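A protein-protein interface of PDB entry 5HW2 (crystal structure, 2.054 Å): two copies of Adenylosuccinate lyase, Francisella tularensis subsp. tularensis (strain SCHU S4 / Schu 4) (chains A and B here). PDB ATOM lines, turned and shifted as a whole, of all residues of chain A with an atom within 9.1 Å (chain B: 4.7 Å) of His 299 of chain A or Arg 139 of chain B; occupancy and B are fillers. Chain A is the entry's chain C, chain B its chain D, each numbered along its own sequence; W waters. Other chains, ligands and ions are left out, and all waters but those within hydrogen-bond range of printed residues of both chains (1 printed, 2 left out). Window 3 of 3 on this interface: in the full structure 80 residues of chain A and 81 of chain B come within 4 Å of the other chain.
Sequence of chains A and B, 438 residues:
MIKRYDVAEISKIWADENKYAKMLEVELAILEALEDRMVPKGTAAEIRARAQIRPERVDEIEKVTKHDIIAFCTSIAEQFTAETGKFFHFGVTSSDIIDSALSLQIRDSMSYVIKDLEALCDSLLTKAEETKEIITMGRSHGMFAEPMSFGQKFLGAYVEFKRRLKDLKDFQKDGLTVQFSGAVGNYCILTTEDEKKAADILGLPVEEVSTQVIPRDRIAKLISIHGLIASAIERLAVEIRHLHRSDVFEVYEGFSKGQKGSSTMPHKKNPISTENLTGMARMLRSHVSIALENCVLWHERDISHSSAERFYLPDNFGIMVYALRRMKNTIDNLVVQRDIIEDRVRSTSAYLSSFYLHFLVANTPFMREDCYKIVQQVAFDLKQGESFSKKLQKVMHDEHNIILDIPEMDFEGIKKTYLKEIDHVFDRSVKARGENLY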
ATOM      1  N   ALA A 183      10.837  22.632 -15.002  1.00  0.00           N
ATOM      2  CA  ALA A 183       9.642  23.463 -14.893  1.00  0.00           C
ATOM      3  C   ALA A 183       8.552  22.806 -14.053  1.00  0.00           C
ATOM      4  O   ALA A 183       8.155  23.349 -13.019  1.00  0.00           O
ATOM      5  CB  ALA A 183       9.103  23.802 -16.285  1.00  0.00           C
ATOM      6  N   VAL A 184       8.061  21.646 -14.476  1.00  0.00           N
ATOM      7  CA  VAL A 184       7.012  20.993 -13.704  1.00  0.00           C
ATOM      8  C   VAL A 184       7.463  19.626 -13.194  1.00  0.00           C
ATOM      9  O   VAL A 184       6.634  18.793 -12.834  1.00  0.00           O
ATOM     10  CB  VAL A 184       5.709  20.885 -14.513  1.00  0.00           C
ATOM     11  CG1 VAL A 184       4.991  22.202 -14.530  1.00  0.00           C
ATOM     12  CG2 VAL A 184       5.985  20.414 -15.913  1.00  0.00           C
ATOM     13  N   GLY A 185       8.772  19.444 -13.055  1.00  0.00           N
ATOM     14  CA  GLY A 185       9.305  18.192 -12.565  1.00  0.00           C
ATOM     15  C   GLY A 185       9.501  17.129 -13.619  1.00  0.00           C
ATOM     16  O   GLY A 185       9.610  15.948 -13.271  1.00  0.00           O
ATOM     17  N   ASN A 186       9.551  17.508 -14.895  1.00  0.00           N
ATOM     18  CA  ASN A 186       9.690  16.563 -15.993  1.00  0.00           C
ATOM     19  C   ASN A 186      11.138  16.260 -16.352  1.00  0.00           C
ATOM     20  O   ASN A 186      11.378  15.358 -17.162  1.00  0.00           O
ATOM     21  CB  ASN A 186       8.962  17.091 -17.232  1.00  0.00           C
ATOM     22  CG  ASN A 186       9.127  18.586 -17.406  1.00  0.00           C
ATOM     23  OD1 ASN A 186       9.833  19.240 -16.639  1.00  0.00           O
ATOM     24  ND2 ASN A 186       8.473  19.137 -18.420  1.00  0.00           N
ATOM     25  N   SER A 210       8.669  15.617  -7.053  1.00  0.00           N
ATOM     26  CA  SER A 210       8.466  17.052  -6.950  1.00  0.00           C
ATOM     27  C   SER A 210       7.836  17.564  -8.235  1.00  0.00           C
ATOM     28  O   SER A 210       8.155  17.085  -9.327  1.00  0.00           O
ATOM     29  CB  SER A 210       9.786  17.786  -6.688  1.00  0.00           C
ATOM     30  OG  SER A 210      10.672  17.646  -7.786  1.00  0.00           O
ATOM     31  N   THR A 211       6.926  18.526  -8.096  1.00  0.00           N
ATOM     32  CA  THR A 211       6.407  19.250  -9.247  1.00  0.00           C
ATOM     33  C   THR A 211       7.341  20.414  -9.544  1.00  0.00           C
ATOM     34  O   THR A 211       8.563  20.236  -9.581  1.00  0.00           O
ATOM     35  CB  THR A 211       4.983  19.741  -8.990  1.00  0.00           C
ATOM     36  OG1 THR A 211       4.971  20.600  -7.841  1.00  0.00           O
ATOM     37  CG2 THR A 211       4.049  18.565  -8.746  1.00  0.00           C
ATOM     38  N   GLN A 212       6.789  21.614  -9.748  1.00  0.00           N
ATOM     39  CA  GLN A 212       7.651  22.787  -9.809  1.00  0.00           C
ATOM     40  C   GLN A 212       8.308  23.048  -8.460  1.00  0.00           C
ATOM     41  O   GLN A 212       9.458  23.500  -8.409  1.00  0.00           O
ATOM     42  CB  GLN A 212       6.867  24.020 -10.281  1.00  0.00           C
ATOM     43  CG  GLN A 212       7.761  25.248 -10.524  1.00  0.00           C
ATOM     44  CD  GLN A 212       7.231  26.191 -11.600  1.00  0.00           C
ATOM     45  OE1 GLN A 212       6.652  27.238 -11.305  1.00  0.00           O
ATOM     46  NE2 GLN A 212       7.426  25.815 -12.855  1.00  0.00           N
ATOM     47  N   VAL A 213       7.617  22.736  -7.366  1.00  0.00           N
ATOM     48  CA  VAL A 213       8.111  22.994  -6.022  1.00  0.00           C
ATOM     49  C   VAL A 213       8.208  21.676  -5.258  1.00  0.00           C
ATOM     50  O   VAL A 213       7.676  20.645  -5.670  1.00  0.00           O
ATOM     51  CB  VAL A 213       7.223  23.995  -5.258  1.00  0.00           C
ATOM     52  CG1 VAL A 213       7.164  25.319  -5.994  1.00  0.00           C
ATOM     53  CG2 VAL A 213       5.831  23.422  -5.068  1.00  0.00           C
ATOM     54  N   CYS A 295      -0.179  23.559   1.942  1.00  0.00           N
ATOM     55  CA  CYS A 295       0.082  22.306   1.238  1.00  0.00           C
ATOM     56  C   CYS A 295      -0.787  22.157  -0.004  1.00  0.00           C
ATOM     57  O   CYS A 295      -0.399  21.459  -0.947  1.00  0.00           O
ATOM     58  CB  CYS A 295      -0.141  21.117   2.172  1.00  0.00           C
ATOM     59  SG  CYS A 295       1.031  20.999   3.526  1.00  0.00           S
ATOM     60  N   VAL A 296      -1.954  22.793  -0.024  1.00  0.00           N
ATOM     61  CA  VAL A 296      -2.928  22.585  -1.112  1.00  0.00           C
ATOM     62  C   VAL A 296      -2.562  23.571  -2.211  1.00  0.00           C
ATOM     63  O   VAL A 296      -3.136  24.654  -2.354  1.00  0.00           O
ATOM     64  CB  VAL A 296      -4.373  22.743  -0.627  1.00  0.00           C
ATOM     65  CG1 VAL A 296      -5.344  22.307  -1.710  1.00  0.00           C
ATOM     66  CG2 VAL A 296      -4.591  21.946   0.648  1.00  0.00           C
ATOM     67  N   LEU A 297      -1.582  23.183  -3.022  1.00  0.00           N
ATOM     68  CA  LEU A 297      -1.197  24.041  -4.131  1.00  0.00           C
ATOM     69  C   LEU A 297      -1.773  23.497  -5.432  1.00  0.00           C
ATOM     70  O   LEU A 297      -1.711  22.290  -5.692  1.00  0.00           O
ATOM     71  CB  LEU A 297       0.326  24.151  -4.234  1.00  0.00           C
ATOM     72  CG  LEU A 297       1.032  24.693  -3.029  1.00  0.00           C
ATOM     73  CD1 LEU A 297       2.447  24.537  -3.137  1.00  0.00           C
ATOM     74  CD2 LEU A 297       0.714  26.102  -2.790  1.00  0.00           C
ATOM     75  N   TRP A 298      -2.250  24.437  -6.246  1.00  0.00           N
ATOM     76  CA  TRP A 298      -2.968  24.089  -7.466  1.00  0.00           C
ATOM     77  C   TRP A 298      -2.027  23.444  -8.475  1.00  0.00           C
ATOM     78  O   TRP A 298      -1.003  24.031  -8.842  1.00  0.00           O
ATOM     79  CB  TRP A 298      -3.622  25.330  -8.071  1.00  0.00           C
ATOM     80  CG  TRP A 298      -4.784  25.864  -7.290  1.00  0.00           C
ATOM     81  CD1 TRP A 298      -5.113  25.572  -5.998  1.00  0.00           C
ATOM     82  CD2 TRP A 298      -5.779  26.780  -7.760  1.00  0.00           C
ATOM     83  NE1 TRP A 298      -6.249  26.253  -5.633  1.00  0.00           N
ATOM     84  CE2 TRP A 298      -6.679  27.001  -6.699  1.00  0.00           C
ATOM     85  CE3 TRP A 298      -5.999  27.432  -8.977  1.00  0.00           C
ATOM     86  CZ2 TRP A 298      -7.777  27.849  -6.816  1.00  0.00           C
ATOM     87  CZ3 TRP A 298      -7.089  28.274  -9.092  1.00  0.00           C
ATOM     88  CH2 TRP A 298      -7.963  28.476  -8.017  1.00  0.00           C
ATOM     89  N   HIS A 299      -2.384  22.240  -8.929  1.00  0.00           N
ATOM     90  CA  HIS A 299      -1.649  21.534  -9.973  1.00  0.00           C
ATOM     91  C   HIS A 299      -0.156  21.465  -9.677  1.00  0.00           C
ATOM     92  O   HIS A 299       0.250  20.983  -8.615  1.00  0.00           O
ATOM     93  CB  HIS A 299      -1.899  22.194 -11.330  1.00  0.00           C
ATOM     94  CG  HIS A 299      -3.201  21.802 -11.958  1.00  0.00           C
ATOM     95  ND1 HIS A 299      -3.706  20.522 -11.881  1.00  0.00           N
ATOM     96  CD2 HIS A 299      -4.102  22.520 -12.668  1.00  0.00           C
ATOM     97  CE1 HIS A 299      -4.861  20.467 -12.521  1.00  0.00           C
ATOM     98  NE2 HIS A 299      -5.124  21.667 -13.007  1.00  0.00           N
ATOM     99  N   GLU A 300       0.671  21.951 -10.603  1.00  0.00           N
ATOM    100  CA  GLU A 300       2.112  21.815 -10.438  1.00  0.00           C
ATOM    101  C   GLU A 300       2.721  22.901  -9.563  1.00  0.00           C
ATOM    102  O   GLU A 300       3.858  22.728  -9.111  1.00  0.00           O
ATOM    103  CB  GLU A 300       2.799  21.795 -11.803  1.00  0.00           C
ATOM    104  CG  GLU A 300       3.128  20.402 -12.282  1.00  0.00           C
ATOM    105  CD  GLU A 300       1.931  19.543 -12.399  1.00  0.00           C
ATOM    106  OE1 GLU A 300       1.164  19.750 -13.282  1.00  0.00           O
ATOM    107  OE2 GLU A 300       1.749  18.660 -11.607  1.00  0.00           O
ATOM    108  N   ARG A 301       2.006  24.003  -9.322  1.00  0.00           N
ATOM    109  CA  ARG A 301       2.368  24.985  -8.300  1.00  0.00           C
ATOM    110  C   ARG A 301       1.417  26.169  -8.366  1.00  0.00           C
ATOM    111  O   ARG A 301       0.774  26.424  -9.389  1.00  0.00           O
ATOM    112  CB  ARG A 301       3.789  25.532  -8.450  1.00  0.00           C
ATOM    113  CG  ARG A 301       3.823  26.854  -9.198  1.00  0.00           C
ATOM    114  CD  ARG A 301       5.009  27.691  -8.817  1.00  0.00           C
ATOM    115  NE  ARG A 301       5.092  28.000  -7.394  1.00  0.00           N
ATOM    116  CZ  ARG A 301       6.198  28.476  -6.838  1.00  0.00           C
ATOM    117  NH1 ARG A 301       7.266  28.660  -7.598  1.00  0.00           N
ATOM    118  NH2 ARG A 301       6.253  28.752  -5.544  1.00  0.00           N
ATOM    119  N   ASP A 302       1.358  26.900  -7.255  1.00  0.00           N
ATOM    120  CA  ASP A 302       0.957  28.298  -7.237  1.00  0.00           C
ATOM    121  C   ASP A 302       1.779  28.988  -6.156  1.00  0.00           C
ATOM    122  O   ASP A 302       2.280  28.344  -5.231  1.00  0.00           O
ATOM    123  CB  ASP A 302      -0.552  28.469  -7.008  1.00  0.00           C
ATOM    124  CG  ASP A 302      -1.040  27.791  -5.745  1.00  0.00           C
ATOM    125  OD1 ASP A 302      -0.824  28.345  -4.649  1.00  0.00           O
ATOM    126  OD2 ASP A 302      -1.655  26.710  -5.849  1.00  0.00           O
ATOM    127  N   MET B 137       0.052  18.438 -20.146  1.00  0.00           N
ATOM    128  CA  MET B 137       0.693  19.739 -20.003  1.00  0.00           C
ATOM    129  C   MET B 137       0.666  20.140 -18.534  1.00  0.00           C
ATOM    130  O   MET B 137      -0.407  20.370 -17.965  1.00  0.00           O
ATOM    131  CB  MET B 137      -0.001  20.785 -20.870  1.00  0.00           C
ATOM    132  CG  MET B 137       0.473  20.789 -22.307  1.00  0.00           C
ATOM    133  SD  MET B 137       2.246  21.093 -22.432  1.00  0.00           S
ATOM    134  CE  MET B 137       2.367  22.723 -21.700  1.00  0.00           C
ATOM    135  N   GLY B 138       1.843  20.210 -17.919  1.00  0.00           N
ATOM    136  CA  GLY B 138       1.926  20.729 -16.569  1.00  0.00           C
ATOM    137  C   GLY B 138       1.443  22.164 -16.499  1.00  0.00           C
ATOM    138  O   GLY B 138       1.586  22.941 -17.447  1.00  0.00           O
ATOM    139  N   ARG B 139       0.847  22.515 -15.364  1.00  0.00           N
ATOM    140  CA  ARG B 139       0.282  23.844 -15.164  1.00  0.00           C
ATOM    141  C   ARG B 139       0.961  24.498 -13.971  1.00  0.00           C
ATOM    142  O   ARG B 139       0.804  24.046 -12.832  1.00  0.00           O
ATOM    143  CB  ARG B 139      -1.232  23.777 -14.972  1.00  0.00           C
ATOM    144  CG  ARG B 139      -1.985  23.434 -16.246  1.00  0.00           C
ATOM    145  CD  ARG B 139      -3.482  23.365 -16.012  1.00  0.00           C
ATOM    146  NE  ARG B 139      -4.180  22.769 -17.148  1.00  0.00           N
ATOM    147  CZ  ARG B 139      -4.267  21.460 -17.362  1.00  0.00           C
ATOM    148  NH1 ARG B 139      -3.694  20.612 -16.518  1.00  0.00           N
ATOM    149  NH2 ARG B 139      -4.922  20.998 -18.419  1.00  0.00           N
ATOM    150  N   SER B 140       1.722  25.554 -14.242  1.00  0.00           N
ATOM    151  CA  SER B 140       2.291  26.411 -13.212  1.00  0.00           C
ATOM    152  C   SER B 140       1.467  27.689 -13.141  1.00  0.00           C
ATOM    153  O   SER B 140       1.257  28.351 -14.162  1.00  0.00           O
ATOM    154  CB  SER B 140       3.754  26.734 -13.515  1.00  0.00           C
ATOM    155  OG  SER B 140       4.370  27.381 -12.416  1.00  0.00           O
ATOM    156  N   HIS B 141       0.994  28.020 -11.937  1.00  0.00           N
ATOM    157  CA  HIS B 141       0.093  29.155 -11.714  1.00  0.00           C
ATOM    158  C   HIS B 141      -1.188  29.024 -12.532  1.00  0.00           C
ATOM    159  O   HIS B 141      -1.840  30.022 -12.847  1.00  0.00           O
ATOM    160  CB  HIS B 141       0.777  30.491 -12.024  1.00  0.00           C
ATOM    161  CG  HIS B 141       2.164  30.602 -11.479  1.00  0.00           C
ATOM    162  ND1 HIS B 141       2.425  30.901 -10.159  1.00  0.00           N
ATOM    163  CD2 HIS B 141       3.370  30.456 -12.077  1.00  0.00           C
ATOM    164  CE1 HIS B 141       3.732  30.933  -9.967  1.00  0.00           C
ATOM    165  NE2 HIS B 141       4.327  30.666 -11.115  1.00  0.00           N
ATOM    166  N   GLY B 142      -1.562  27.793 -12.876  1.00  0.00           N
ATOM    167  CA  GLY B 142      -2.668  27.566 -13.780  1.00  0.00           C
ATOM    168  C   GLY B 142      -2.344  27.781 -15.240  1.00  0.00           C
ATOM    169  O   GLY B 142      -3.222  27.573 -16.087  1.00  0.00           O
ATOM    170  N   MET B 143      -1.122  28.194 -15.563  1.00  0.00           N
ATOM    171  CA  MET B 143      -0.702  28.388 -16.941  1.00  0.00           C
ATOM    172  C   MET B 143      -0.001  27.145 -17.460  1.00  0.00           C
ATOM    173  O   MET B 143       0.711  26.461 -16.720  1.00  0.00           O
ATOM    174  CB  MET B 143       0.254  29.572 -17.072  1.00  0.00           C
ATOM    175  CG  MET B 143      -0.285  30.892 -16.600  1.00  0.00           C
ATOM    176  SD  MET B 143      -1.932  31.244 -17.210  1.00  0.00           S
ATOM    177  CE  MET B 143      -2.770  31.351 -15.645  1.00  0.00           C
ATOM    178  N   PHE B 144      -0.191  26.870 -18.748  1.00  0.00           N
ATOM    179  CA  PHE B 144       0.585  25.831 -19.411  1.00  0.00           C
ATOM    180  C   PHE B 144       2.072  26.093 -19.218  1.00  0.00           C
ATOM    181  O   PHE B 144       2.547  27.217 -19.402  1.00  0.00           O
ATOM    182  CB  PHE B 144       0.248  25.787 -20.903  1.00  0.00           C
ATOM    183  CG  PHE B 144      -1.150  25.328 -21.198  1.00  0.00           C
ATOM    184  CD1 PHE B 144      -1.836  24.528 -20.301  1.00  0.00           C
ATOM    185  CD2 PHE B 144      -1.777  25.696 -22.376  1.00  0.00           C
ATOM    186  CE1 PHE B 144      -3.123  24.106 -20.572  1.00  0.00           C
ATOM    187  CE2 PHE B 144      -3.064  25.278 -22.652  1.00  0.00           C
ATOM    188  CZ  PHE B 144      -3.738  24.484 -21.749  1.00  0.00           C
ATOM    189  N   ALA B 145       2.803  25.052 -18.828  1.00  0.00           N
ATOM    190  CA  ALA B 145       4.240  25.182 -18.633  1.00  0.00           C
ATOM    191  C   ALA B 145       4.990  24.283 -19.605  1.00  0.00           C
ATOM    192  O   ALA B 145       5.403  24.732 -20.679  1.00  0.00           O
ATOM    193  CB  ALA B 145       4.623  24.855 -17.190  1.00  0.00           C
ATOM    194  N   LYS B 153       1.093  13.115 -11.464  1.00  0.00           N
ATOM    195  CA  LYS B 153       0.082  13.732 -10.613  1.00  0.00           C
ATOM    196  C   LYS B 153      -0.419  12.748  -9.563  1.00  0.00           C
ATOM    197  O   LYS B 153      -0.654  13.124  -8.408  1.00  0.00           O
ATOM    198  CB  LYS B 153      -1.074  14.251 -11.468  1.00  0.00           C
ATOM    199  CG  LYS B 153      -0.681  15.356 -12.436  1.00  0.00           C
ATOM    200  CD  LYS B 153      -1.849  15.754 -13.323  1.00  0.00           C
ATOM    201  CE  LYS B 153      -1.498  16.941 -14.206  1.00  0.00           C
ATOM    202  NZ  LYS B 153      -1.294  18.189 -13.416  1.00  0.00           N
ATOM    203  N   GLU B 239      -6.682  18.583  -6.921  1.00  0.00           N
ATOM    204  CA  GLU B 239      -6.133  18.122  -8.192  1.00  0.00           C
ATOM    205  C   GLU B 239      -7.222  17.505  -9.061  1.00  0.00           C
ATOM    206  O   GLU B 239      -7.326  17.805 -10.256  1.00  0.00           O
ATOM    207  CB  GLU B 239      -5.010  17.116  -7.942  1.00  0.00           C
ATOM    208  CG  GLU B 239      -4.332  16.628  -9.207  1.00  0.00           C
ATOM    209  CD  GLU B 239      -3.485  17.700  -9.859  1.00  0.00           C
ATOM    210  OE1 GLU B 239      -2.823  18.463  -9.123  1.00  0.00           O
ATOM    211  OE2 GLU B 239      -3.485  17.785 -11.105  1.00  0.00           O
ATOM    212  N   HIS B 242      -9.835  20.168 -10.181  1.00  0.00           N
ATOM    213  CA  HIS B 242      -9.320  20.988 -11.273  1.00  0.00           C
ATOM    214  C   HIS B 242      -9.456  20.271 -12.610  1.00  0.00           C
ATOM    215  O   HIS B 242      -9.980  20.831 -13.579  1.00  0.00           O
ATOM    216  CB  HIS B 242      -7.859  21.354 -11.008  1.00  0.00           C
ATOM    217  CG  HIS B 242      -7.685  22.587 -10.178  1.00  0.00           C
ATOM    218  ND1 HIS B 242      -8.516  23.681 -10.286  1.00  0.00           N
ATOM    219  CD2 HIS B 242      -6.772  22.900  -9.228  1.00  0.00           C
ATOM    220  CE1 HIS B 242      -8.122  24.615  -9.439  1.00  0.00           C
ATOM    221  NE2 HIS B 242      -7.068  24.166  -8.783  1.00  0.00           N
ATOM    222  N   LEU B 243      -8.989  19.025 -12.681  1.00  0.00           N
ATOM    223  CA  LEU B 243      -9.065  18.346 -13.967  1.00  0.00           C
ATOM    224  C   LEU B 243     -10.463  17.838 -14.289  1.00  0.00           C
ATOM    225  O   LEU B 243     -10.705  17.427 -15.430  1.00  0.00           O
ATOM    226  CB  LEU B 243      -8.066  17.189 -13.996  1.00  0.00           C
ATOM    227  CG  LEU B 243      -6.635  17.568 -13.781  1.00  0.00           C
ATOM    228  CD1 LEU B 243      -5.853  16.451 -13.355  1.00  0.00           C
ATOM    229  CD2 LEU B 243      -6.043  18.146 -14.986  1.00  0.00           C
ATOM    230  N   VAL B 248     -11.365  21.896 -18.424  1.00  0.00           N
ATOM    231  CA  VAL B 248     -10.292  20.910 -18.479  1.00  0.00           C
ATOM    232  C   VAL B 248     -10.860  19.616 -19.051  1.00  0.00           C
ATOM    233  O   VAL B 248     -10.402  19.135 -20.093  1.00  0.00           O
ATOM    234  CB  VAL B 248      -9.664  20.704 -17.089  1.00  0.00           C
ATOM    235  CG1 VAL B 248      -8.435  19.838 -17.182  1.00  0.00           C
ATOM    236  CG2 VAL B 248      -9.298  22.043 -16.485  1.00  0.00           C
ATOM    237  N   GLU B 250     -10.835  16.438 -18.386  1.00  0.00           N
ATOM    238  CA  GLU B 250      -9.984  15.281 -18.644  1.00  0.00           C
ATOM    239  C   GLU B 250     -10.238  14.111 -17.706  1.00  0.00           C
ATOM    240  O   GLU B 250      -9.832  12.987 -18.026  1.00  0.00           O
ATOM    241  CB  GLU B 250      -8.507  15.685 -18.571  1.00  0.00           C
ATOM    242  CG  GLU B 250      -8.259  17.093 -18.918  1.00  0.00           C
ATOM    243  CD  GLU B 250      -6.789  17.436 -19.072  1.00  0.00           C
ATOM    244  OE1 GLU B 250      -6.415  18.022 -20.067  1.00  0.00           O
ATOM    245  OE2 GLU B 250      -5.998  17.102 -18.213  1.00  0.00           O
ATOM    246  N   ARG B 344      -4.345  18.170 -25.705  1.00  0.00           N
ATOM    247  CA  ARG B 344      -3.934  19.465 -25.180  1.00  0.00           C
ATOM    248  C   ARG B 344      -2.433  19.673 -25.334  1.00  0.00           C
ATOM    249  O   ARG B 344      -1.976  20.811 -25.474  1.00  0.00           O
ATOM    250  CB  ARG B 344      -4.359  19.592 -23.715  1.00  0.00           C
ATOM    251  CG  ARG B 344      -4.001  20.918 -23.068  1.00  0.00           C
ATOM    252  CD  ARG B 344      -4.844  21.186 -21.831  1.00  0.00           C
ATOM    253  NE  ARG B 344      -6.153  21.740 -22.169  1.00  0.00           N
ATOM    254  CZ  ARG B 344      -7.307  21.111 -21.979  1.00  0.00           C
ATOM    255  NH1 ARG B 344      -7.326  19.900 -21.440  1.00  0.00           N
ATOM    256  NH2 ARG B 344      -8.446  21.700 -22.319  1.00  0.00           N
HETATM  257  O   HOH W   1      -4.335  20.732  -7.560  1.00  0.00           O
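OG1 of Thr 211 of chain A is in hydrogen-bond range of O of Glu 300 of chain A, at 2.7 Å.
The backbone NH (N) of Gln 212 of chain A sits at hydrogen-bond distance from the backbone carbonyl oxygen (O) of Glu 300 of chain A, at 3.2 Å.
The backbone carbonyl oxygen of Gly 138 of chain B sits at hydrogen-bond distance from the backbone NH of Ala 145 of chain B (2.8 Å).
The guanidinium group of Arg 139 of chain B is in salt-bridge range of the side-chain carboxylate of Glu 250 of chain B, at 3.7 Å.
NZ of Lys 153 of chain B lies within salt-bridge range of OE2 of Glu 239 of chain B, at 3.2 Å.
The backbone NH (N) of Glu 250 of chain B is in hydrogen-bond range of the backbone carbonyl oxygen (O) of Leu 243 of chain B (3.1 Å).
Among the printed residues, pairs that only touch across the chains: Val 184 of chain A with Gly 138 of chain B, Val 184 of chain A with Ala 145 of chain B, Trp 298 of chain A with His 242 of chain B, His 299 of chain A with Arg 139 of chain B, His 299 of chain A with Lys 153 of chain B, His 299 of chain A with His 242 of chain B, His 299 of chain A with Leu 243 of chain B, Glu 300 of chain A with Gly 138 of chain B, Arg 301 of chain A with Arg 139 of chain B and Arg 301 of chain A with Ser 140 of chain B.
Water W1 bridges the backbone NH (N) of His 299 of chain A (2.8 Å) and the side-chain carboxylate (OE1) of Glu 239 of chain B (3.1 Å).
The side-chain hydroxyl of Ser 140 of chain B sits at hydrogen-bond distance from the side-chain amide oxygen of Gln 212 of chain A.
ND1 of His 299 of chain A sits at hydrogen-bond distance from OE2 of Glu 239 of chain B.
The backbone carbonyl oxygen (O) of Arg 139 of chain B lies within hydrogen-bond range of the backbone NH (N) of Glu 300 of chain A, at 3.1 Å.
The side-chain carboxylate of Glu 300 of chain A lies within salt-bridge range of the side-chain amino group of Lys 153 of chain B (2.9 Å).
N of His 141 of chain B is in hydrogen-bond range of O of Arg 301 of chain A (3.0 Å).
Printed residues of chain B within 4 Å of Gln 212 of chain A: Ser 140 (2.5 Å).
Printed residues of chain B within 4 Å of His 299 of chain A: Arg 139 (3.5 Å), Lys 153 (3.7 Å), Glu 239 (2.9 Å), His 242 (3.4 Å) and Leu 243 (3.6 Å).
Of chain A, only His 299 (3.5 Å), Glu 300 (3.1 Å) and Arg 301 (3.7 Å) come within 4 Å of Arg 139 of chain B.
Of the printed residues of chain A, His 141 of chain B touches Arg 301.
No residue of chain A comes within 4 Å of Gly 142 of chain B.
Of the printed residues of chain A, Ala 145 of chain B touches Val 184 (3.8 Å).
Of the printed residues of chain A, His 242 of chain B touches Trp 298 and His 299.
The nearest residue of chain A that does not touch Arg 139 of chain B is Val 184 of chain A (4.2 Å).
No position is printed for both chains.
Of the 16 printed residues of chain B, 9 touch a printed residue of chain A.
Hydrophobic or aromatic side chains of chain B that line the printed part of chain A: His 141, Ala 145, His 242 and Leu 243.
Hydrophobic or aromatic side chains of chain A that line the printed part of chain B: Val 184, Trp 298 and His 299.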
